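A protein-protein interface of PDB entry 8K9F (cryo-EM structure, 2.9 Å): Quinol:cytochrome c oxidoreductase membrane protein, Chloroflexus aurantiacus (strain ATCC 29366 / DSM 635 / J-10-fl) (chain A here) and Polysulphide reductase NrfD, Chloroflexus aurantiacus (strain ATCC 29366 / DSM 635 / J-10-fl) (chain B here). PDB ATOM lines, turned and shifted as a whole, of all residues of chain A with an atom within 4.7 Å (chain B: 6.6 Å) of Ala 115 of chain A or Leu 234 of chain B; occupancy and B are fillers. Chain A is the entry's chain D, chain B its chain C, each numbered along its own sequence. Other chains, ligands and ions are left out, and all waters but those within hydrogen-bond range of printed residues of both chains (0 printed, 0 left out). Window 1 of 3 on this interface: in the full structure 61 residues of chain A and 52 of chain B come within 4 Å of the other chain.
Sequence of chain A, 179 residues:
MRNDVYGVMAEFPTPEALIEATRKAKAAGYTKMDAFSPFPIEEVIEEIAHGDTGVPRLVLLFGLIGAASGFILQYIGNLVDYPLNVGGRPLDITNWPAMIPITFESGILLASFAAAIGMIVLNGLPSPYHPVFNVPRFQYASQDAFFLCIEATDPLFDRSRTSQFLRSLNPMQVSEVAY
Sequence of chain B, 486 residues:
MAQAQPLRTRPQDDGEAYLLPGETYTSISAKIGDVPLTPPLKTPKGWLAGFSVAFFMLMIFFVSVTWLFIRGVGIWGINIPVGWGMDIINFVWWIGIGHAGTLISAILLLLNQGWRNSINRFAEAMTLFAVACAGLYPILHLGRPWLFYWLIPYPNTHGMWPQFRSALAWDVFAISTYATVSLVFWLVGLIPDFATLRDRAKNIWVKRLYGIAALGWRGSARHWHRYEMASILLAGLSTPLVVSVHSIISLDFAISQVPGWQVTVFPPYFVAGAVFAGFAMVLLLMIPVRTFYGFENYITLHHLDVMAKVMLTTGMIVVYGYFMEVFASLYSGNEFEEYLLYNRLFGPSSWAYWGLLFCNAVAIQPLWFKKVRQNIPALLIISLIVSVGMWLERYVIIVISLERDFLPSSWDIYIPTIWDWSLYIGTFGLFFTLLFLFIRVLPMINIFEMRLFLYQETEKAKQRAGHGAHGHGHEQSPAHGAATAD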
ATOM      1  N   VAL A  59     -15.523   7.479  16.602  1.00  0.00           N
ATOM      2  CA  VAL A  59     -16.419   6.811  17.543  1.00  0.00           C
ATOM      3  C   VAL A  59     -15.834   5.460  17.950  1.00  0.00           C
ATOM      4  O   VAL A  59     -15.947   5.057  19.111  1.00  0.00           O
ATOM      5  CB  VAL A  59     -17.855   6.690  16.979  1.00  0.00           C
ATOM      6  CG1 VAL A  59     -17.887   6.037  15.696  1.00  0.00           C
ATOM      7  CG2 VAL A  59     -18.778   5.968  17.892  1.00  0.00           C
ATOM      8  N   ALA A 111     -18.535   7.237  23.059  1.00  0.00           N
ATOM      9  CA  ALA A 111     -18.761   7.029  21.638  1.00  0.00           C
ATOM     10  C   ALA A 111     -19.735   8.046  21.053  1.00  0.00           C
ATOM     11  O   ALA A 111     -19.523   8.542  19.942  1.00  0.00           O
ATOM     12  CB  ALA A 111     -19.275   5.608  21.446  1.00  0.00           C
ATOM     13  N   SER A 112     -20.792   8.391  21.789  1.00  0.00           N
ATOM     14  CA  SER A 112     -21.770   9.344  21.277  1.00  0.00           C
ATOM     15  C   SER A 112     -21.267  10.776  21.372  1.00  0.00           C
ATOM     16  O   SER A 112     -21.592  11.600  20.506  1.00  0.00           O
ATOM     17  CB  SER A 112     -23.087   9.190  22.021  1.00  0.00           C
ATOM     18  OG  SER A 112     -23.640   7.904  21.805  1.00  0.00           O
ATOM     19  N   PHE A 113     -20.486  11.090  22.419  1.00  0.00           N
ATOM     20  CA  PHE A 113     -19.745  12.349  22.433  1.00  0.00           C
ATOM     21  C   PHE A 113     -18.824  12.458  21.230  1.00  0.00           C
ATOM     22  O   PHE A 113     -18.724  13.527  20.614  1.00  0.00           O
ATOM     23  CB  PHE A 113     -18.907  12.486  23.700  1.00  0.00           C
ATOM     24  CG  PHE A 113     -19.608  13.147  24.839  1.00  0.00           C
ATOM     25  CD1 PHE A 113     -20.632  12.513  25.505  1.00  0.00           C
ATOM     26  CD2 PHE A 113     -19.220  14.414  25.255  1.00  0.00           C
ATOM     27  CE1 PHE A 113     -21.246  13.115  26.563  1.00  0.00           C
ATOM     28  CE2 PHE A 113     -19.850  15.031  26.318  1.00  0.00           C
ATOM     29  CZ  PHE A 113     -20.867  14.380  26.970  1.00  0.00           C
ATOM     30  N   ALA A 114     -18.147  11.356  20.885  1.00  0.00           N
ATOM     31  CA  ALA A 114     -17.274  11.338  19.718  1.00  0.00           C
ATOM     32  C   ALA A 114     -18.053  11.575  18.437  1.00  0.00           C
ATOM     33  O   ALA A 114     -17.632  12.368  17.598  1.00  0.00           O
ATOM     34  CB  ALA A 114     -16.532  10.011  19.638  1.00  0.00           C
ATOM     35  N   ALA A 115     -19.212  10.929  18.293  1.00  0.00           N
ATOM     36  CA  ALA A 115     -20.007  11.080  17.076  1.00  0.00           C
ATOM     37  C   ALA A 115     -20.525  12.506  16.920  1.00  0.00           C
ATOM     38  O   ALA A 115     -20.335  13.130  15.866  1.00  0.00           O
ATOM     39  CB  ALA A 115     -21.158  10.077  17.076  1.00  0.00           C
ATOM     40  N   ALA A 116     -21.105  13.063  17.992  1.00  0.00           N
ATOM     41  CA  ALA A 116     -21.627  14.427  17.965  1.00  0.00           C
ATOM     42  C   ALA A 116     -20.528  15.452  17.722  1.00  0.00           C
ATOM     43  O   ALA A 116     -20.566  16.202  16.737  1.00  0.00           O
ATOM     44  CB  ALA A 116     -22.330  14.741  19.280  1.00  0.00           C
ATOM     45  N   ILE A 117     -19.537  15.492  18.617  1.00  0.00           N
ATOM     46  CA  ILE A 117     -18.498  16.510  18.559  1.00  0.00           C
ATOM     47  C   ILE A 117     -17.604  16.303  17.340  1.00  0.00           C
ATOM     48  O   ILE A 117     -17.160  17.275  16.727  1.00  0.00           O
ATOM     49  CB  ILE A 117     -17.738  16.518  19.904  1.00  0.00           C
ATOM     50  CG1 ILE A 117     -18.633  17.141  20.984  1.00  0.00           C
ATOM     51  CG2 ILE A 117     -16.384  17.233  19.823  1.00  0.00           C
ATOM     52  CD1 ILE A 117     -17.929  17.532  22.278  1.00  0.00           C
ATOM     53  N   GLY A 118     -17.398  15.059  16.904  1.00  0.00           N
ATOM     54  CA  GLY A 118     -16.586  14.820  15.728  1.00  0.00           C
ATOM     55  C   GLY A 118     -17.272  15.210  14.437  1.00  0.00           C
ATOM     56  O   GLY A 118     -16.624  15.712  13.521  1.00  0.00           O
ATOM     57  N   MET A 119     -18.586  14.988  14.336  1.00  0.00           N
ATOM     58  CA  MET A 119     -19.304  15.484  13.167  1.00  0.00           C
ATOM     59  C   MET A 119     -19.366  17.010  13.157  1.00  0.00           C
ATOM     60  O   MET A 119     -19.144  17.640  12.115  1.00  0.00           O
ATOM     61  CB  MET A 119     -20.706  14.885  13.120  1.00  0.00           C
ATOM     62  CG  MET A 119     -21.495  15.465  12.000  1.00  0.00           C
ATOM     63  SD  MET A 119     -22.809  16.453  12.672  1.00  0.00           S
ATOM     64  CE  MET A 119     -23.653  16.827  11.171  1.00  0.00           C
ATOM     65  N   ALA B 106     -34.014   5.812  16.691  1.00  0.00           N
ATOM     66  CA  ALA B 106     -32.783   5.118  16.347  1.00  0.00           C
ATOM     67  C   ALA B 106     -33.015   3.787  15.654  1.00  0.00           C
ATOM     68  O   ALA B 106     -32.347   3.498  14.652  1.00  0.00           O
ATOM     69  CB  ALA B 106     -31.943   4.905  17.614  1.00  0.00           C
ATOM     70  N   LEU B 109     -34.411   4.121  12.273  1.00  0.00           N
ATOM     71  CA  LEU B 109     -33.346   4.666  11.440  1.00  0.00           C
ATOM     72  C   LEU B 109     -32.396   3.568  11.001  1.00  0.00           C
ATOM     73  O   LEU B 109     -31.861   3.605   9.887  1.00  0.00           O
ATOM     74  CB  LEU B 109     -32.592   5.756  12.197  1.00  0.00           C
ATOM     75  CG  LEU B 109     -31.553   6.550  11.411  1.00  0.00           C
ATOM     76  CD1 LEU B 109     -32.140   6.995  10.083  1.00  0.00           C
ATOM     77  CD2 LEU B 109     -31.062   7.740  12.207  1.00  0.00           C
ATOM     78  N   VAL B 181     -27.270  10.907  25.542  1.00  0.00           N
ATOM     79  CA  VAL B 181     -27.325  10.437  24.159  1.00  0.00           C
ATOM     80  C   VAL B 181     -28.636  10.847  23.497  1.00  0.00           C
ATOM     81  O   VAL B 181     -28.649  11.249  22.329  1.00  0.00           O
ATOM     82  CB  VAL B 181     -27.097   8.915  24.091  1.00  0.00           C
ATOM     83  CG1 VAL B 181     -27.334   8.375  22.681  1.00  0.00           C
ATOM     84  CG2 VAL B 181     -25.680   8.582  24.497  1.00  0.00           C
ATOM     85  N   VAL B 184     -28.253  14.416  22.703  1.00  0.00           N
ATOM     86  CA  VAL B 184     -27.355  14.557  21.558  1.00  0.00           C
ATOM     87  C   VAL B 184     -28.075  14.228  20.255  1.00  0.00           C
ATOM     88  O   VAL B 184     -27.943  14.949  19.258  1.00  0.00           O
ATOM     89  CB  VAL B 184     -26.107  13.681  21.777  1.00  0.00           C
ATOM     90  CG1 VAL B 184     -25.448  13.294  20.474  1.00  0.00           C
ATOM     91  CG2 VAL B 184     -25.107  14.418  22.645  1.00  0.00           C
ATOM     92  N   PHE B 185     -28.862  13.151  20.252  1.00  0.00           N
ATOM     93  CA  PHE B 185     -29.622  12.769  19.068  1.00  0.00           C
ATOM     94  C   PHE B 185     -30.668  13.819  18.722  1.00  0.00           C
ATOM     95  O   PHE B 185     -30.870  14.129  17.545  1.00  0.00           O
ATOM     96  CB  PHE B 185     -30.285  11.407  19.278  1.00  0.00           C
ATOM     97  CG  PHE B 185     -30.189  10.496  18.085  1.00  0.00           C
ATOM     98  CD1 PHE B 185     -29.474  10.875  16.959  1.00  0.00           C
ATOM     99  CD2 PHE B 185     -30.812   9.258  18.090  1.00  0.00           C
ATOM    100  CE1 PHE B 185     -29.385  10.043  15.859  1.00  0.00           C
ATOM    101  CE2 PHE B 185     -30.724   8.418  16.996  1.00  0.00           C
ATOM    102  CZ  PHE B 185     -30.007   8.812  15.877  1.00  0.00           C
ATOM    103  N   VAL B 188     -28.534  16.946  17.166  1.00  0.00           N
ATOM    104  CA  VAL B 188     -28.140  16.729  15.774  1.00  0.00           C
ATOM    105  C   VAL B 188     -29.362  16.556  14.876  1.00  0.00           C
ATOM    106  O   VAL B 188     -29.356  17.022  13.734  1.00  0.00           O
ATOM    107  CB  VAL B 188     -27.143  15.563  15.624  1.00  0.00           C
ATOM    108  CG1 VAL B 188     -26.384  15.702  14.329  1.00  0.00           C
ATOM    109  CG2 VAL B 188     -26.116  15.612  16.719  1.00  0.00           C
ATOM    110  N   ARG B 226     -21.479  13.548   6.422  1.00  0.00           N
ATOM    111  CA  ARG B 226     -21.230  13.371   7.840  1.00  0.00           C
ATOM    112  C   ARG B 226     -22.519  13.413   8.642  1.00  0.00           C
ATOM    113  O   ARG B 226     -22.591  12.780   9.697  1.00  0.00           O
ATOM    114  CB  ARG B 226     -20.246  14.432   8.318  1.00  0.00           C
ATOM    115  CG  ARG B 226     -18.881  14.269   7.677  1.00  0.00           C
ATOM    116  CD  ARG B 226     -17.769  14.802   8.551  1.00  0.00           C
ATOM    117  NE  ARG B 226     -16.513  14.905   7.818  1.00  0.00           N
ATOM    118  CZ  ARG B 226     -16.197  15.892   6.989  1.00  0.00           C
ATOM    119  NH1 ARG B 226     -17.029  16.889   6.747  1.00  0.00           N
ATOM    120  NH2 ARG B 226     -15.015  15.874   6.386  1.00  0.00           N
ATOM    121  N   MET B 229     -24.069   9.979   8.163  1.00  0.00           N
ATOM    122  CA  MET B 229     -23.102   9.004   8.601  1.00  0.00           C
ATOM    123  C   MET B 229     -23.126   8.960  10.131  1.00  0.00           C
ATOM    124  O   MET B 229     -23.286   7.889  10.734  1.00  0.00           O
ATOM    125  CB  MET B 229     -21.763   9.498   8.061  1.00  0.00           C
ATOM    126  CG  MET B 229     -20.540   9.247   8.828  1.00  0.00           C
ATOM    127  SD  MET B 229     -20.411   7.479   9.017  1.00  0.00           S
ATOM    128  CE  MET B 229     -20.240   7.170   7.244  1.00  0.00           C
ATOM    129  N   ALA B 230     -23.087  10.144  10.761  1.00  0.00           N
ATOM    130  CA  ALA B 230     -23.150  10.265  12.207  1.00  0.00           C
ATOM    131  C   ALA B 230     -24.527   9.931  12.750  1.00  0.00           C
ATOM    132  O   ALA B 230     -24.625   9.418  13.860  1.00  0.00           O
ATOM    133  CB  ALA B 230     -22.759  11.676  12.630  1.00  0.00           C
ATOM    134  N   SER B 231     -25.598  10.213  12.005  1.00  0.00           N
ATOM    135  CA  SER B 231     -26.934   9.906  12.503  1.00  0.00           C
ATOM    136  C   SER B 231     -27.219   8.412  12.451  1.00  0.00           C
ATOM    137  O   SER B 231     -27.801   7.863  13.389  1.00  0.00           O
ATOM    138  CB  SER B 231     -27.987  10.668  11.707  1.00  0.00           C
ATOM    139  OG  SER B 231     -28.237  10.032  10.469  1.00  0.00           O
ATOM    140  N   ILE B 232     -26.795   7.741  11.373  1.00  0.00           N
ATOM    141  CA  ILE B 232     -26.927   6.288  11.268  1.00  0.00           C
ATOM    142  C   ILE B 232     -26.070   5.619  12.332  1.00  0.00           C
ATOM    143  O   ILE B 232     -26.493   4.666  12.997  1.00  0.00           O
ATOM    144  CB  ILE B 232     -26.549   5.819   9.839  1.00  0.00           C
ATOM    145  CG1 ILE B 232     -27.724   5.834   8.837  1.00  0.00           C
ATOM    146  CG2 ILE B 232     -25.907   4.427   9.825  1.00  0.00           C
ATOM    147  CD1 ILE B 232     -28.661   7.034   8.810  1.00  0.00           C
ATOM    148  N   LEU B 233     -24.872   6.129  12.520  1.00  0.00           N
ATOM    149  CA  LEU B 233     -23.946   5.574  13.509  1.00  0.00           C
ATOM    150  C   LEU B 233     -24.357   5.839  14.939  1.00  0.00           C
ATOM    151  O   LEU B 233     -24.062   5.054  15.811  1.00  0.00           O
ATOM    152  CB  LEU B 233     -22.586   6.186  13.264  1.00  0.00           C
ATOM    153  CG  LEU B 233     -21.402   5.976  14.174  1.00  0.00           C
ATOM    154  CD1 LEU B 233     -20.523   4.933  13.515  1.00  0.00           C
ATOM    155  CD2 LEU B 233     -20.704   7.321  14.224  1.00  0.00           C
ATOM    156  N   LEU B 234     -25.034   6.938  15.178  1.00  0.00           N
ATOM    157  CA  LEU B 234     -25.507   7.248  16.539  1.00  0.00           C
ATOM    158  C   LEU B 234     -26.731   6.442  16.770  1.00  0.00           C
ATOM    159  O   LEU B 234     -27.012   6.077  17.895  1.00  0.00           O
ATOM    160  CB  LEU B 234     -25.849   8.724  16.715  1.00  0.00           C
ATOM    161  CG  LEU B 234     -24.899   9.560  17.563  1.00  0.00           C
ATOM    162  CD1 LEU B 234     -24.892  11.005  17.089  1.00  0.00           C
ATOM    163  CD2 LEU B 234     -25.315   9.460  19.018  1.00  0.00           C
ATOM    164  N   ALA B 235     -27.541   6.233  15.745  1.00  0.00           N
ATOM    165  CA  ALA B 235     -28.630   5.277  15.891  1.00  0.00           C
ATOM    166  C   ALA B 235     -28.085   3.901  16.226  1.00  0.00           C
ATOM    167  O   ALA B 235     -28.652   3.184  17.052  1.00  0.00           O
ATOM    168  CB  ALA B 235     -29.464   5.229  14.613  1.00  0.00           C
ATOM    169  N   GLY B 236     -26.968   3.527  15.603  1.00  0.00           N
ATOM    170  CA  GLY B 236     -26.272   2.304  15.943  1.00  0.00           C
ATOM    171  C   GLY B 236     -25.681   2.283  17.333  1.00  0.00           C
ATOM    172  O   GLY B 236     -25.429   1.201  17.862  1.00  0.00           O
ATOM    173  N   LEU B 237     -25.389   3.447  17.906  1.00  0.00           N
ATOM    174  CA  LEU B 237     -24.991   3.505  19.308  1.00  0.00           C
ATOM    175  C   LEU B 237     -26.169   3.468  20.270  1.00  0.00           C
ATOM    176  O   LEU B 237     -26.087   2.814  21.315  1.00  0.00           O
ATOM    177  CB  LEU B 237     -24.194   4.774  19.592  1.00  0.00           C
ATOM    178  CG  LEU B 237     -22.791   4.814  19.010  1.00  0.00           C
ATOM    179  CD1 LEU B 237     -22.232   6.208  19.192  1.00  0.00           C
ATOM    180  CD2 LEU B 237     -21.906   3.751  19.619  1.00  0.00           C
ATOM    181  N   SER B 238     -27.247   4.187  19.961  1.00  0.00           N
ATOM    182  CA  SER B 238     -28.390   4.305  20.852  1.00  0.00           C
ATOM    183  C   SER B 238     -29.333   3.117  20.785  1.00  0.00           C
ATOM    184  O   SER B 238     -30.099   2.906  21.729  1.00  0.00           O
ATOM    185  CB  SER B 238     -29.176   5.580  20.538  1.00  0.00           C
ATOM    186  OG  SER B 238     -29.865   6.043  21.684  1.00  0.00           O
ATOM    187  N   THR B 239     -29.306   2.356  19.693  1.00  0.00           N
ATOM    188  CA  THR B 239     -30.138   1.160  19.583  1.00  0.00           C
ATOM    189  C   THR B 239     -29.810   0.069  20.606  1.00  0.00           C
ATOM    190  O   THR B 239     -30.749  -0.371  21.293  1.00  0.00           O
ATOM    191  CB  THR B 239     -30.100   0.645  18.140  1.00  0.00           C
ATOM    192  OG1 THR B 239     -30.823   1.546  17.288  1.00  0.00           O
ATOM    193  CG2 THR B 239     -30.702  -0.740  18.040  1.00  0.00           C
ATOM    194  N   PRO B 240     -28.557  -0.396  20.803  1.00  0.00           N
ATOM    195  CA  PRO B 240     -28.321  -1.306  21.939  1.00  0.00           C
ATOM    196  C   PRO B 240     -28.464  -0.611  23.284  1.00  0.00           C
ATOM    197  O   PRO B 240     -28.767  -1.274  24.288  1.00  0.00           O
ATOM    198  CB  PRO B 240     -26.876  -1.759  21.737  1.00  0.00           C
ATOM    199  CG  PRO B 240     -26.216  -0.619  21.109  1.00  0.00           C
ATOM    200  CD  PRO B 240     -27.253  -0.041  20.183  1.00  0.00           C
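Of the 10 printed residues of chain A, 6 touch a printed residue of chain B. Along chain A the printed residues that touch a printed residue of chain B span positions 59 to 119. Of the 19 printed residues of chain B, 7 touch a printed residue of chain A. Printed residues of chain B that touch a printed residue of chain A: Val 181, Val 184, Arg 226, Ala 230, Leu 233, Leu 234 and Leu 237. Hydrophobic or aromatic side chains of chain B that line the printed part of chain A: Val 181, Val 184, Ala 230, Leu 233, Leu 234 and Leu 237. Among the printed residues, 11 pairs touch across the chains. Among the printed residues, no Asp or Glu carboxylate lies within 4 Å of a Lys or Arg side-chain nitrogen of the other chain.
Of the printed residues of chain B, Ala 115 of chain A touches Leu 233 and Leu 234. Of the printed residues of chain B, Ala 111 of chain A touches Leu 237 (3.6 Å). Of the printed residues of chain A, Leu 233 of chain B touches Val 59 (3.4 Å) and Ala 115 (3.99 Å). Pro 240 of chain B touches none of the printed residues of chain A. The nearest residue of chain A that does not touch Leu 234 of chain B is Ala 116 of chain A (4.4 Å). The nearest printed residue of chain A that does not touch Val 181 of chain B is Phe 113 of chain A (6.1 Å).
CD2 of Leu 233 of chain B touches CG1 of Val 59 of chain A, 3.4 Å away. CG2 of Val 59 of chain A touches CD1 of Leu 237 of chain B (3.7 Å). Ala 111 of chain A touches Leu 237 of chain B. OG of Ser 112 of chain A touches CG2 of Val 181 of chain B, at 3.4 Å. Leu 237 of chain B touches Ser 112 of chain A (CD1 to OG, 3.4 Å). CD2 of Leu 233 of chain B touches CB of Ala 115 of chain A, 3.99 Å away. Leu 234 of chain B touches Ala 115 of chain A (CG to CB, 3.8 Å). Val 184 of chain B touches Ala 116 of chain A. Met 119 of chain A touches Arg 226 of chain B. CB of Met 119 of chain A touches CB of Ala 230 of chain B, at 3.8 Å.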
